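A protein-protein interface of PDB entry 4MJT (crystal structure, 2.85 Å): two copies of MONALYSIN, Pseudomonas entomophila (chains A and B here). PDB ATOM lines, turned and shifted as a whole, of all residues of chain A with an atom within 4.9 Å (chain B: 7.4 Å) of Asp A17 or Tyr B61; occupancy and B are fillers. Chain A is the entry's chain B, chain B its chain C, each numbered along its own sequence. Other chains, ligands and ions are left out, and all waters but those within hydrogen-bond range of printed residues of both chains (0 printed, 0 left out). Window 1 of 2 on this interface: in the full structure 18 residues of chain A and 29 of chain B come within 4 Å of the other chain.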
ATOM      1  N   ASP A  13      17.671  27.190   6.424  1.00  0.00           N
ATOM      2  CA  ASP A  13      18.985  27.789   6.581  1.00  0.00           C
ATOM      3  C   ASP A  13      20.152  26.855   6.191  1.00  0.00           C
ATOM      4  O   ASP A  13      21.073  27.319   5.530  1.00  0.00           O
ATOM      5  CB  ASP A  13      19.147  28.288   8.020  1.00  0.00           C
ATOM      6  CG  ASP A  13      18.808  29.737   8.270  1.00  0.00           C
ATOM      7  OD1 ASP A  13      18.602  30.475   7.283  1.00  0.00           O
ATOM      8  OD2 ASP A  13      18.864  30.164   9.449  1.00  0.00           O
ATOM      9  N   PHE A  14      20.113  25.555   6.580  1.00  0.00           N
ATOM     10  CA  PHE A  14      21.174  24.592   6.258  1.00  0.00           C
ATOM     11  C   PHE A  14      21.458  24.505   4.747  1.00  0.00           C
ATOM     12  O   PHE A  14      22.624  24.568   4.339  1.00  0.00           O
ATOM     13  CB  PHE A  14      20.876  23.205   6.865  1.00  0.00           C
ATOM     14  CG  PHE A  14      21.892  22.139   6.524  1.00  0.00           C
ATOM     15  CD1 PHE A  14      23.098  22.050   7.224  1.00  0.00           C
ATOM     16  CD2 PHE A  14      21.643  21.221   5.507  1.00  0.00           C
ATOM     17  CE1 PHE A  14      24.044  21.078   6.896  1.00  0.00           C
ATOM     18  CE2 PHE A  14      22.582  20.245   5.184  1.00  0.00           C
ATOM     19  CZ  PHE A  14      23.776  20.176   5.881  1.00  0.00           C
ATOM     20  N   ALA A  15      20.381  24.355   3.935  1.00  0.00           N
ATOM     21  CA  ALA A  15      20.433  24.269   2.477  1.00  0.00           C
ATOM     22  C   ALA A  15      20.807  25.617   1.846  1.00  0.00           C
ATOM     23  O   ALA A  15      21.676  25.646   0.972  1.00  0.00           O
ATOM     24  CB  ALA A  15      19.102  23.791   1.947  1.00  0.00           C
ATOM     25  N   ILE A  16      20.172  26.729   2.296  1.00  0.00           N
ATOM     26  CA  ILE A  16      20.431  28.080   1.790  1.00  0.00           C
ATOM     27  C   ILE A  16      21.876  28.519   2.072  1.00  0.00           C
ATOM     28  O   ILE A  16      22.607  28.830   1.130  1.00  0.00           O
ATOM     29  CB  ILE A  16      19.381  29.116   2.283  1.00  0.00           C
ATOM     30  CG1 ILE A  16      17.946  28.721   1.852  1.00  0.00           C
ATOM     31  CG2 ILE A  16      19.737  30.518   1.770  1.00  0.00           C
ATOM     32  CD1 ILE A  16      16.865  29.329   2.687  1.00  0.00           C
ATOM     33  N   ASP A  17      22.284  28.530   3.363  1.00  0.00           N
ATOM     34  CA  ASP A  17      23.623  28.923   3.810  1.00  0.00           C
ATOM     35  C   ASP A  17      24.706  28.040   3.201  1.00  0.00           C
ATOM     36  O   ASP A  17      25.734  28.552   2.771  1.00  0.00           O
ATOM     37  CB  ASP A  17      23.733  28.913   5.344  1.00  0.00           C
ATOM     38  CG  ASP A  17      22.795  29.835   6.110  1.00  0.00           C
ATOM     39  OD1 ASP A  17      22.014  30.576   5.459  1.00  0.00           O
ATOM     40  OD2 ASP A  17      22.843  29.816   7.361  1.00  0.00           O
ATOM     41  N   GLY A  18      24.455  26.732   3.149  1.00  0.00           N
ATOM     42  CA  GLY A  18      25.376  25.763   2.573  1.00  0.00           C
ATOM     43  C   GLY A  18      25.671  26.062   1.120  1.00  0.00           C
ATOM     44  O   GLY A  18      26.829  26.035   0.695  1.00  0.00           O
ATOM     45  N   TYR A  19      24.621  26.417   0.374  1.00  0.00           N
ATOM     46  CA  TYR A  19      24.699  26.753  -1.040  1.00  0.00           C
ATOM     47  C   TYR A  19      25.425  28.090  -1.294  1.00  0.00           C
ATOM     48  O   TYR A  19      26.428  28.113  -2.001  1.00  0.00           O
ATOM     49  CB  TYR A  19      23.287  26.731  -1.667  1.00  0.00           C
ATOM     50  CG  TYR A  19      23.277  26.993  -3.153  1.00  0.00           C
ATOM     51  CD1 TYR A  19      23.778  26.054  -4.050  1.00  0.00           C
ATOM     52  CD2 TYR A  19      22.767  28.179  -3.667  1.00  0.00           C
ATOM     53  CE1 TYR A  19      23.783  26.295  -5.423  1.00  0.00           C
ATOM     54  CE2 TYR A  19      22.755  28.428  -5.039  1.00  0.00           C
ATOM     55  CZ  TYR A  19      23.263  27.479  -5.914  1.00  0.00           C
ATOM     56  OH  TYR A  19      23.266  27.717  -7.266  1.00  0.00           O
ATOM     57  N   LEU A  20      24.929  29.185  -0.709  1.00  0.00           N
ATOM     58  CA  LEU A  20      25.468  30.531  -0.910  1.00  0.00           C
ATOM     59  C   LEU A  20      26.820  30.774  -0.269  1.00  0.00           C
ATOM     60  O   LEU A  20      27.685  31.360  -0.914  1.00  0.00           O
ATOM     61  CB  LEU A  20      24.462  31.617  -0.461  1.00  0.00           C
ATOM     62  CG  LEU A  20      23.073  31.600  -1.101  1.00  0.00           C
ATOM     63  CD1 LEU A  20      22.134  32.535  -0.368  1.00  0.00           C
ATOM     64  CD2 LEU A  20      23.136  31.974  -2.564  1.00  0.00           C
ATOM     65  N   LEU A  21      27.008  30.338   0.989  1.00  0.00           N
ATOM     66  CA  LEU A  21      28.261  30.559   1.714  1.00  0.00           C
ATOM     67  C   LEU A  21      29.345  29.514   1.368  1.00  0.00           C
ATOM     68  O   LEU A  21      29.643  28.601   2.146  1.00  0.00           O
ATOM     69  CB  LEU A  21      28.019  30.685   3.227  1.00  0.00           C
ATOM     70  CG  LEU A  21      26.878  31.618   3.643  1.00  0.00           C
ATOM     71  CD1 LEU A  21      26.572  31.457   5.107  1.00  0.00           C
ATOM     72  CD2 LEU A  21      27.192  33.068   3.303  1.00  0.00           C
ATOM     73  N   GLN A 184      20.798  39.070   6.557  1.00  0.00           N
ATOM     74  CA  GLN A 184      21.084  38.071   7.580  1.00  0.00           C
ATOM     75  C   GLN A 184      22.464  38.333   8.133  1.00  0.00           C
ATOM     76  O   GLN A 184      23.313  38.878   7.417  1.00  0.00           O
ATOM     77  CB  GLN A 184      21.039  36.663   6.994  1.00  0.00           C
ATOM     78  CG  GLN A 184      19.653  36.229   6.605  1.00  0.00           C
ATOM     79  CD  GLN A 184      19.548  34.743   6.560  1.00  0.00           C
ATOM     80  OE1 GLN A 184      19.167  34.100   7.534  1.00  0.00           O
ATOM     81  NE2 GLN A 184      19.792  34.180   5.400  1.00  0.00           N
ATOM     82  N   LYS A 186      25.072  36.915   8.171  1.00  0.00           N
ATOM     83  CA  LYS A 186      25.798  35.908   7.397  1.00  0.00           C
ATOM     84  C   LYS A 186      26.560  36.585   6.265  1.00  0.00           C
ATOM     85  O   LYS A 186      25.974  37.334   5.482  1.00  0.00           O
ATOM     86  CB  LYS A 186      24.830  34.854   6.820  1.00  0.00           C
ATOM     87  CG  LYS A 186      24.120  34.036   7.875  1.00  0.00           C
ATOM     88  CD  LYS A 186      22.855  33.417   7.347  1.00  0.00           C
ATOM     89  CE  LYS A 186      22.029  32.835   8.461  1.00  0.00           C
ATOM     90  NZ  LYS A 186      20.947  31.982   7.922  1.00  0.00           N
ATOM     91  N   TYR B  58      17.539  15.029  18.789  1.00  0.00           N
ATOM     92  CA  TYR B  58      18.054  15.313  17.454  1.00  0.00           C
ATOM     93  C   TYR B  58      18.941  16.561  17.411  1.00  0.00           C
ATOM     94  O   TYR B  58      18.879  17.391  18.315  1.00  0.00           O
ATOM     95  CB  TYR B  58      16.896  15.391  16.442  1.00  0.00           C
ATOM     96  CG  TYR B  58      16.074  16.660  16.496  1.00  0.00           C
ATOM     97  CD1 TYR B  58      14.984  16.773  17.357  1.00  0.00           C
ATOM     98  CD2 TYR B  58      16.326  17.717  15.619  1.00  0.00           C
ATOM     99  CE1 TYR B  58      14.196  17.921  17.379  1.00  0.00           C
ATOM    100  CE2 TYR B  58      15.547  18.870  15.635  1.00  0.00           C
ATOM    101  CZ  TYR B  58      14.483  18.970  16.519  1.00  0.00           C
ATOM    102  OH  TYR B  58      13.713  20.109  16.541  1.00  0.00           O
ATOM    103  N   LEU B  59      19.752  16.689  16.350  1.00  0.00           N
ATOM    104  CA  LEU B  59      20.640  17.825  16.125  1.00  0.00           C
ATOM    105  C   LEU B  59      19.903  18.940  15.374  1.00  0.00           C
ATOM    106  O   LEU B  59      19.524  18.763  14.217  1.00  0.00           O
ATOM    107  CB  LEU B  59      21.920  17.415  15.367  1.00  0.00           C
ATOM    108  CG  LEU B  59      22.942  16.537  16.091  1.00  0.00           C
ATOM    109  CD1 LEU B  59      24.105  16.205  15.162  1.00  0.00           C
ATOM    110  CD2 LEU B  59      23.510  17.227  17.330  1.00  0.00           C
ATOM    111  N   GLN B  60      19.677  20.068  16.052  1.00  0.00           N
ATOM    112  CA  GLN B  60      19.035  21.255  15.496  1.00  0.00           C
ATOM    113  C   GLN B  60      20.115  22.122  14.860  1.00  0.00           C
ATOM    114  O   GLN B  60      21.185  22.299  15.442  1.00  0.00           O
ATOM    115  CB  GLN B  60      18.320  22.031  16.622  1.00  0.00           C
ATOM    116  CG  GLN B  60      17.799  23.415  16.253  1.00  0.00           C
ATOM    117  CD  GLN B  60      16.772  23.879  17.238  1.00  0.00           C
ATOM    118  OE1 GLN B  60      15.575  23.643  17.065  1.00  0.00           O
ATOM    119  NE2 GLN B  60      17.211  24.558  18.283  1.00  0.00           N
ATOM    120  N   TYR B  61      19.829  22.678  13.683  1.00  0.00           N
ATOM    121  CA  TYR B  61      20.781  23.544  12.993  1.00  0.00           C
ATOM    122  C   TYR B  61      20.948  24.879  13.726  1.00  0.00           C
ATOM    123  O   TYR B  61      19.958  25.449  14.208  1.00  0.00           O
ATOM    124  CB  TYR B  61      20.339  23.758  11.545  1.00  0.00           C
ATOM    125  CG  TYR B  61      21.181  24.732  10.759  1.00  0.00           C
ATOM    126  CD1 TYR B  61      22.342  24.319  10.114  1.00  0.00           C
ATOM    127  CD2 TYR B  61      20.770  26.051  10.584  1.00  0.00           C
ATOM    128  CE1 TYR B  61      23.098  25.207   9.346  1.00  0.00           C
ATOM    129  CE2 TYR B  61      21.527  26.951   9.834  1.00  0.00           C
ATOM    130  CZ  TYR B  61      22.676  26.520   9.196  1.00  0.00           C
ATOM    131  OH  TYR B  61      23.402  27.420   8.453  1.00  0.00           O
ATOM    132  N   VAL B  62      22.209  25.367  13.806  1.00  0.00           N
ATOM    133  CA  VAL B  62      22.556  26.644  14.425  1.00  0.00           C
ATOM    134  C   VAL B  62      23.084  27.636  13.377  1.00  0.00           C
ATOM    135  O   VAL B  62      22.433  28.655  13.136  1.00  0.00           O
ATOM    136  CB  VAL B  62      23.500  26.488  15.649  1.00  0.00           C
ATOM    137  CG1 VAL B  62      24.031  27.834  16.136  1.00  0.00           C
ATOM    138  CG2 VAL B  62      22.807  25.745  16.782  1.00  0.00           C
ATOM    139  N   GLU B  63      24.250  27.338  12.747  1.00  0.00           N
ATOM    140  CA  GLU B  63      24.907  28.257  11.807  1.00  0.00           C
ATOM    141  C   GLU B  63      25.923  27.550  10.908  1.00  0.00           C
ATOM    142  O   GLU B  63      26.431  26.491  11.260  1.00  0.00           O
ATOM    143  CB  GLU B  63      25.659  29.352  12.624  1.00  0.00           C
ATOM    144  CG  GLU B  63      25.846  30.702  11.938  1.00  0.00           C
ATOM    145  CD  GLU B  63      26.510  31.810  12.750  1.00  0.00           C
ATOM    146  OE1 GLU B  63      27.090  31.514  13.818  1.00  0.00           O
ATOM    147  OE2 GLU B  63      26.458  32.983  12.309  1.00  0.00           O
ATOM    148  N   THR B  64      26.226  28.170   9.751  1.00  0.00           N
ATOM    149  CA  THR B  64      27.252  27.763   8.798  1.00  0.00           C
ATOM    150  C   THR B  64      28.358  28.824   8.914  1.00  0.00           C
ATOM    151  O   THR B  64      28.083  30.016   8.820  1.00  0.00           O
ATOM    152  CB  THR B  64      26.690  27.583   7.361  1.00  0.00           C
ATOM    153  OG1 THR B  64      25.689  26.566   7.348  1.00  0.00           O
ATOM    154  CG2 THR B  64      27.771  27.202   6.349  1.00  0.00           C
ATOM    155  N   ILE B  65      29.589  28.386   9.171  1.00  0.00           N
ATOM    156  CA  ILE B  65      30.754  29.246   9.347  1.00  0.00           C
ATOM    157  C   ILE B  65      31.725  29.069   8.185  1.00  0.00           C
ATOM    158  O   ILE B  65      32.035  27.938   7.811  1.00  0.00           O
ATOM    159  CB  ILE B  65      31.400  29.008  10.759  1.00  0.00           C
ATOM    160  CG1 ILE B  65      30.789  29.937  11.821  1.00  0.00           C
ATOM    161  CG2 ILE B  65      32.931  29.175  10.759  1.00  0.00           C
ATOM    162  CD1 ILE B  65      29.451  29.581  12.293  1.00  0.00           C
ATOM    163  N   GLN B  78      25.478  31.930  18.444  1.00  0.00           N
ATOM    164  CA  GLN B  78      24.582  31.913  19.578  1.00  0.00           C
ATOM    165  C   GLN B  78      23.615  30.748  19.576  1.00  0.00           C
ATOM    166  O   GLN B  78      23.034  30.391  18.549  1.00  0.00           O
ATOM    167  CB  GLN B  78      23.864  33.235  19.834  1.00  0.00           C
ATOM    168  CG  GLN B  78      23.389  34.026  18.655  1.00  0.00           C
ATOM    169  CD  GLN B  78      22.915  35.363  19.164  1.00  0.00           C
ATOM    170  OE1 GLN B  78      23.321  35.832  20.246  1.00  0.00           O
ATOM    171  NE2 GLN B  78      22.042  36.009  18.401  1.00  0.00           N
ATOM    172  N   THR B 137      34.682  25.330   5.602  1.00  0.00           N
ATOM    173  CA  THR B 137      33.290  25.665   5.893  1.00  0.00           C
ATOM    174  C   THR B 137      32.807  24.664   6.940  1.00  0.00           C
ATOM    175  O   THR B 137      33.114  23.475   6.844  1.00  0.00           O
ATOM    176  CB  THR B 137      32.454  25.751   4.614  1.00  0.00           C
ATOM    177  OG1 THR B 137      33.081  26.679   3.724  1.00  0.00           O
ATOM    178  CG2 THR B 137      31.026  26.216   4.878  1.00  0.00           C
ATOM    179  N   PHE B 138      32.122  25.155   7.977  1.00  0.00           N
ATOM    180  CA  PHE B 138      31.681  24.338   9.109  1.00  0.00           C
ATOM    181  C   PHE B 138      30.233  24.574   9.449  1.00  0.00           C
ATOM    182  O   PHE B 138      29.711  25.655   9.199  1.00  0.00           O
ATOM    183  CB  PHE B 138      32.560  24.621  10.348  1.00  0.00           C
ATOM    184  CG  PHE B 138      34.044  24.500  10.090  1.00  0.00           C
ATOM    185  CD1 PHE B 138      34.776  25.590   9.613  1.00  0.00           C
ATOM    186  CD2 PHE B 138      34.703  23.287  10.278  1.00  0.00           C
ATOM    187  CE1 PHE B 138      36.138  25.469   9.334  1.00  0.00           C
ATOM    188  CE2 PHE B 138      36.063  23.171  10.012  1.00  0.00           C
ATOM    189  CZ  PHE B 138      36.774  24.265   9.541  1.00  0.00           C
ATOM    190  N   VAL B 139      29.579  23.550  10.017  1.00  0.00           N
ATOM    191  CA  VAL B 139      28.170  23.601  10.405  1.00  0.00           C
ATOM    192  C   VAL B 139      28.096  23.340  11.902  1.00  0.00           C
ATOM    193  O   VAL B 139      28.763  22.427  12.399  1.00  0.00           O
ATOM    194  CB  VAL B 139      27.276  22.626   9.565  1.00  0.00           C
ATOM    195  CG1 VAL B 139      25.799  22.760   9.931  1.00  0.00           C
ATOM    196  CG2 VAL B 139      27.468  22.843   8.067  1.00  0.00           C
ATOM    197  N   ILE B 140      27.320  24.165  12.620  1.00  0.00           N
ATOM    198  CA  ILE B 140      27.112  24.048  14.067  1.00  0.00           C
ATOM    199  C   ILE B 140      25.698  23.545  14.306  1.00  0.00           C
ATOM    200  O   ILE B 140      24.746  24.068  13.717  1.00  0.00           O
ATOM    201  CB  ILE B 140      27.396  25.389  14.828  1.00  0.00           C
ATOM    202  CG1 ILE B 140      28.790  25.942  14.491  1.00  0.00           C
ATOM    203  CG2 ILE B 140      27.195  25.243  16.363  1.00  0.00           C
ATOM    204  CD1 ILE B 140      29.070  27.292  15.052  1.00  0.00           C
ATOM    205  N   TYR B 141      25.570  22.531  15.164  1.00  0.00           N
ATOM    206  CA  TYR B 141      24.295  21.940  15.576  1.00  0.00           C
ATOM    207  C   TYR B 141      24.200  21.981  17.099  1.00  0.00           C
ATOM    208  O   TYR B 141      25.222  21.902  17.775  1.00  0.00           O
ATOM    209  CB  TYR B 141      24.185  20.470  15.143  1.00  0.00           C
ATOM    210  CG  TYR B 141      24.423  20.188  13.674  1.00  0.00           C
ATOM    211  CD1 TYR B 141      25.698  19.892  13.200  1.00  0.00           C
ATOM    212  CD2 TYR B 141      23.356  20.093  12.779  1.00  0.00           C
ATOM    213  CE1 TYR B 141      25.914  19.567  11.863  1.00  0.00           C
ATOM    214  CE2 TYR B 141      23.563  19.775  11.437  1.00  0.00           C
ATOM    215  CZ  TYR B 141      24.845  19.508  10.987  1.00  0.00           C
ATOM    216  OH  TYR B 141      25.079  19.180   9.679  1.00  0.00           O
ATOM    217  N   GLN B 142      22.975  22.058  17.637  1.00  0.00           N
ATOM    218  CA  GLN B 142      22.712  22.035  19.075  1.00  0.00           C
ATOM    219  C   GLN B 142      21.715  20.915  19.349  1.00  0.00           C
ATOM    220  O   GLN B 142      20.749  20.753  18.602  1.00  0.00           O
ATOM    221  CB  GLN B 142      22.182  23.385  19.588  1.00  0.00           C
ATOM    222  CG  GLN B 142      22.054  23.473  21.114  1.00  0.00           C
ATOM    223  CD  GLN B 142      21.589  24.817  21.613  1.00  0.00           C
ATOM    224  OE1 GLN B 142      21.231  25.720  20.849  1.00  0.00           O
ATOM    225  NE2 GLN B 142      21.532  24.960  22.923  1.00  0.00           N
ATOM    226  N   VAL B 144      18.707  18.866  20.821  1.00  0.00           N
ATOM    227  CA  VAL B 144      17.330  19.117  21.229  1.00  0.00           C
ATOM    228  C   VAL B 144      16.775  17.813  21.823  1.00  0.00           C
ATOM    229  O   VAL B 144      17.001  16.738  21.251  1.00  0.00           O
ATOM    230  CB  VAL B 144      16.479  19.610  20.031  1.00  0.00           C
ATOM    231  CG1 VAL B 144      14.999  19.656  20.382  1.00  0.00           C
ATOM    232  CG2 VAL B 144      16.949  20.971  19.544  1.00  0.00           C
ATOM    233  N   VAL B 196      25.506  16.629   8.010  1.00  0.00           N
ATOM    234  CA  VAL B 196      24.284  15.865   7.788  1.00  0.00           C
ATOM    235  C   VAL B 196      23.083  16.832   7.695  1.00  0.00           C
ATOM    236  O   VAL B 196      23.102  17.883   8.329  1.00  0.00           O
ATOM    237  CB  VAL B 196      24.130  14.774   8.891  1.00  0.00           C
ATOM    238  CG1 VAL B 196      23.664  15.354  10.227  1.00  0.00           C
ATOM    239  CG2 VAL B 196      23.219  13.644   8.431  1.00  0.00           C
ATOM    240  N   THR B 197      22.062  16.491   6.896  1.00  0.00           N
ATOM    241  CA  THR B 197      20.857  17.317   6.767  1.00  0.00           C
ATOM    242  C   THR B 197      20.105  17.291   8.109  1.00  0.00           C
ATOM    243  O   THR B 197      19.730  16.214   8.562  1.00  0.00           O
ATOM    244  CB  THR B 197      19.988  16.848   5.584  1.00  0.00           C
ATOM    245  OG1 THR B 197      20.771  16.845   4.389  1.00  0.00           O
ATOM    246  CG2 THR B 197      18.757  17.715   5.384  1.00  0.00           C
ATOM    247  N   PRO B 198      19.909  18.444   8.788  1.00  0.00           N
ATOM    248  CA  PRO B 198      19.216  18.407  10.085  1.00  0.00           C
ATOM    249  C   PRO B 198      17.718  18.188   9.956  1.00  0.00           C
ATOM    250  O   PRO B 198      17.098  18.639   8.990  1.00  0.00           O
ATOM    251  CB  PRO B 198      19.528  19.779  10.694  1.00  0.00           C
ATOM    252  CG  PRO B 198      19.716  20.662   9.537  1.00  0.00           C
ATOM    253  CD  PRO B 198      20.295  19.821   8.429  1.00  0.00           C
ATOM    254  N   LEU B 199      17.141  17.487  10.932  1.00  0.00           N
ATOM    255  CA  LEU B 199      15.704  17.271  11.008  1.00  0.00           C
ATOM    256  C   LEU B 199      15.111  18.572  11.553  1.00  0.00           C
ATOM    257  O   LEU B 199      15.793  19.306  12.277  1.00  0.00           O
ATOM    258  CB  LEU B 199      15.382  16.130  11.996  1.00  0.00           C
ATOM    259  CG  LEU B 199      15.743  14.702  11.598  1.00  0.00           C
ATOM    260  CD1 LEU B 199      15.818  13.806  12.834  1.00  0.00           C
ATOM    261  CD2 LEU B 199      14.742  14.136  10.605  1.00  0.00           C
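No position is printed for both chains.
Ile A16 touches none of the printed residues of chain B.
Asp A17 touches just these residues of chain B: Tyr B61 (2.7 Å) and Thr B64 (3.7 Å).
Gln B60 touches none of the printed residues of chain A.
Of chain A, only Asp A13, Phe A14 and Asp A17 come within 4 Å of Tyr B61.
Printed residues of chain A within 4 Å of Thr B64: Asp A17.
Printed residues of chain A within 4 Å of Thr B137: Leu A21 (3.9 Å).
The nearest printed residue of chain A that does not touch Tyr B61 is Lys A186 (5.2 Å).
Asp A13 touches Tyr B61.
CE1 of Tyr B61 touches CA of Phe A14 (3.7 Å).
Val B139 touches Phe A14 (CG1 to CE1, 3.9 Å).
Phe A14 touches Tyr B141 (CE1 to OH, 3.5 Å).
Phe A14 touches Val B196 (CZ to O, 3.4 Å).
Phe A14 touches Thr B197 (CE2 to CA, 3.7 Å).
CD of Pro B198 touches CG of Phe A14, at 3.4 Å.
Thr B64 touches Asp A17 (OG1 to CB, 3.7 Å).
Thr B137 touches Leu A21 (CG2 to O, 3.9 Å).
The side-chain amino group of Lys A186 lies within salt-bridge range of the side-chain carboxylate of Asp A13 (2.9 Å).
The side-chain hydroxyl of Tyr B141 lies within hydrogen-bond range of the backbone carbonyl oxygen of Val B196 (2.7 Å).
The side-chain amino group (NZ) of Lys A186 lies within salt-bridge range of the side-chain carboxylate (OD2) of Asp A17, 2.9 Å away.
The side-chain hydroxyl of Tyr B61 sits at hydrogen-bond distance from the side-chain hydroxyl of Thr B64 (2.7 Å).
Printed residues of chain B that touch a printed residue of chain A: Tyr B61, Thr B64, Thr B137, Val B139, Tyr B141, Val B196, Thr B197 and Pro B198.
Hydrophobic or aromatic side chains of chain B that line the printed part of chain A: Tyr B61, Val B139, Tyr B141 and Pro B198.
Printed residues of chain A that touch a printed residue of chain B: Asp A13, Phe A14, Asp A17 and Leu A21.
Hydrophobic or aromatic side chains of chain A that line the printed part of chain B: Phe A14.
Among the printed residues, no Asp or Glu carboxylate lies within 4 Å of a Lys or Arg side-chain nitrogen of the other chain.
The side-chain carboxylate of Asp A17 lies within hydrogen-bond range of the side-chain hydroxyl of Tyr B61 (2.7 Å).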
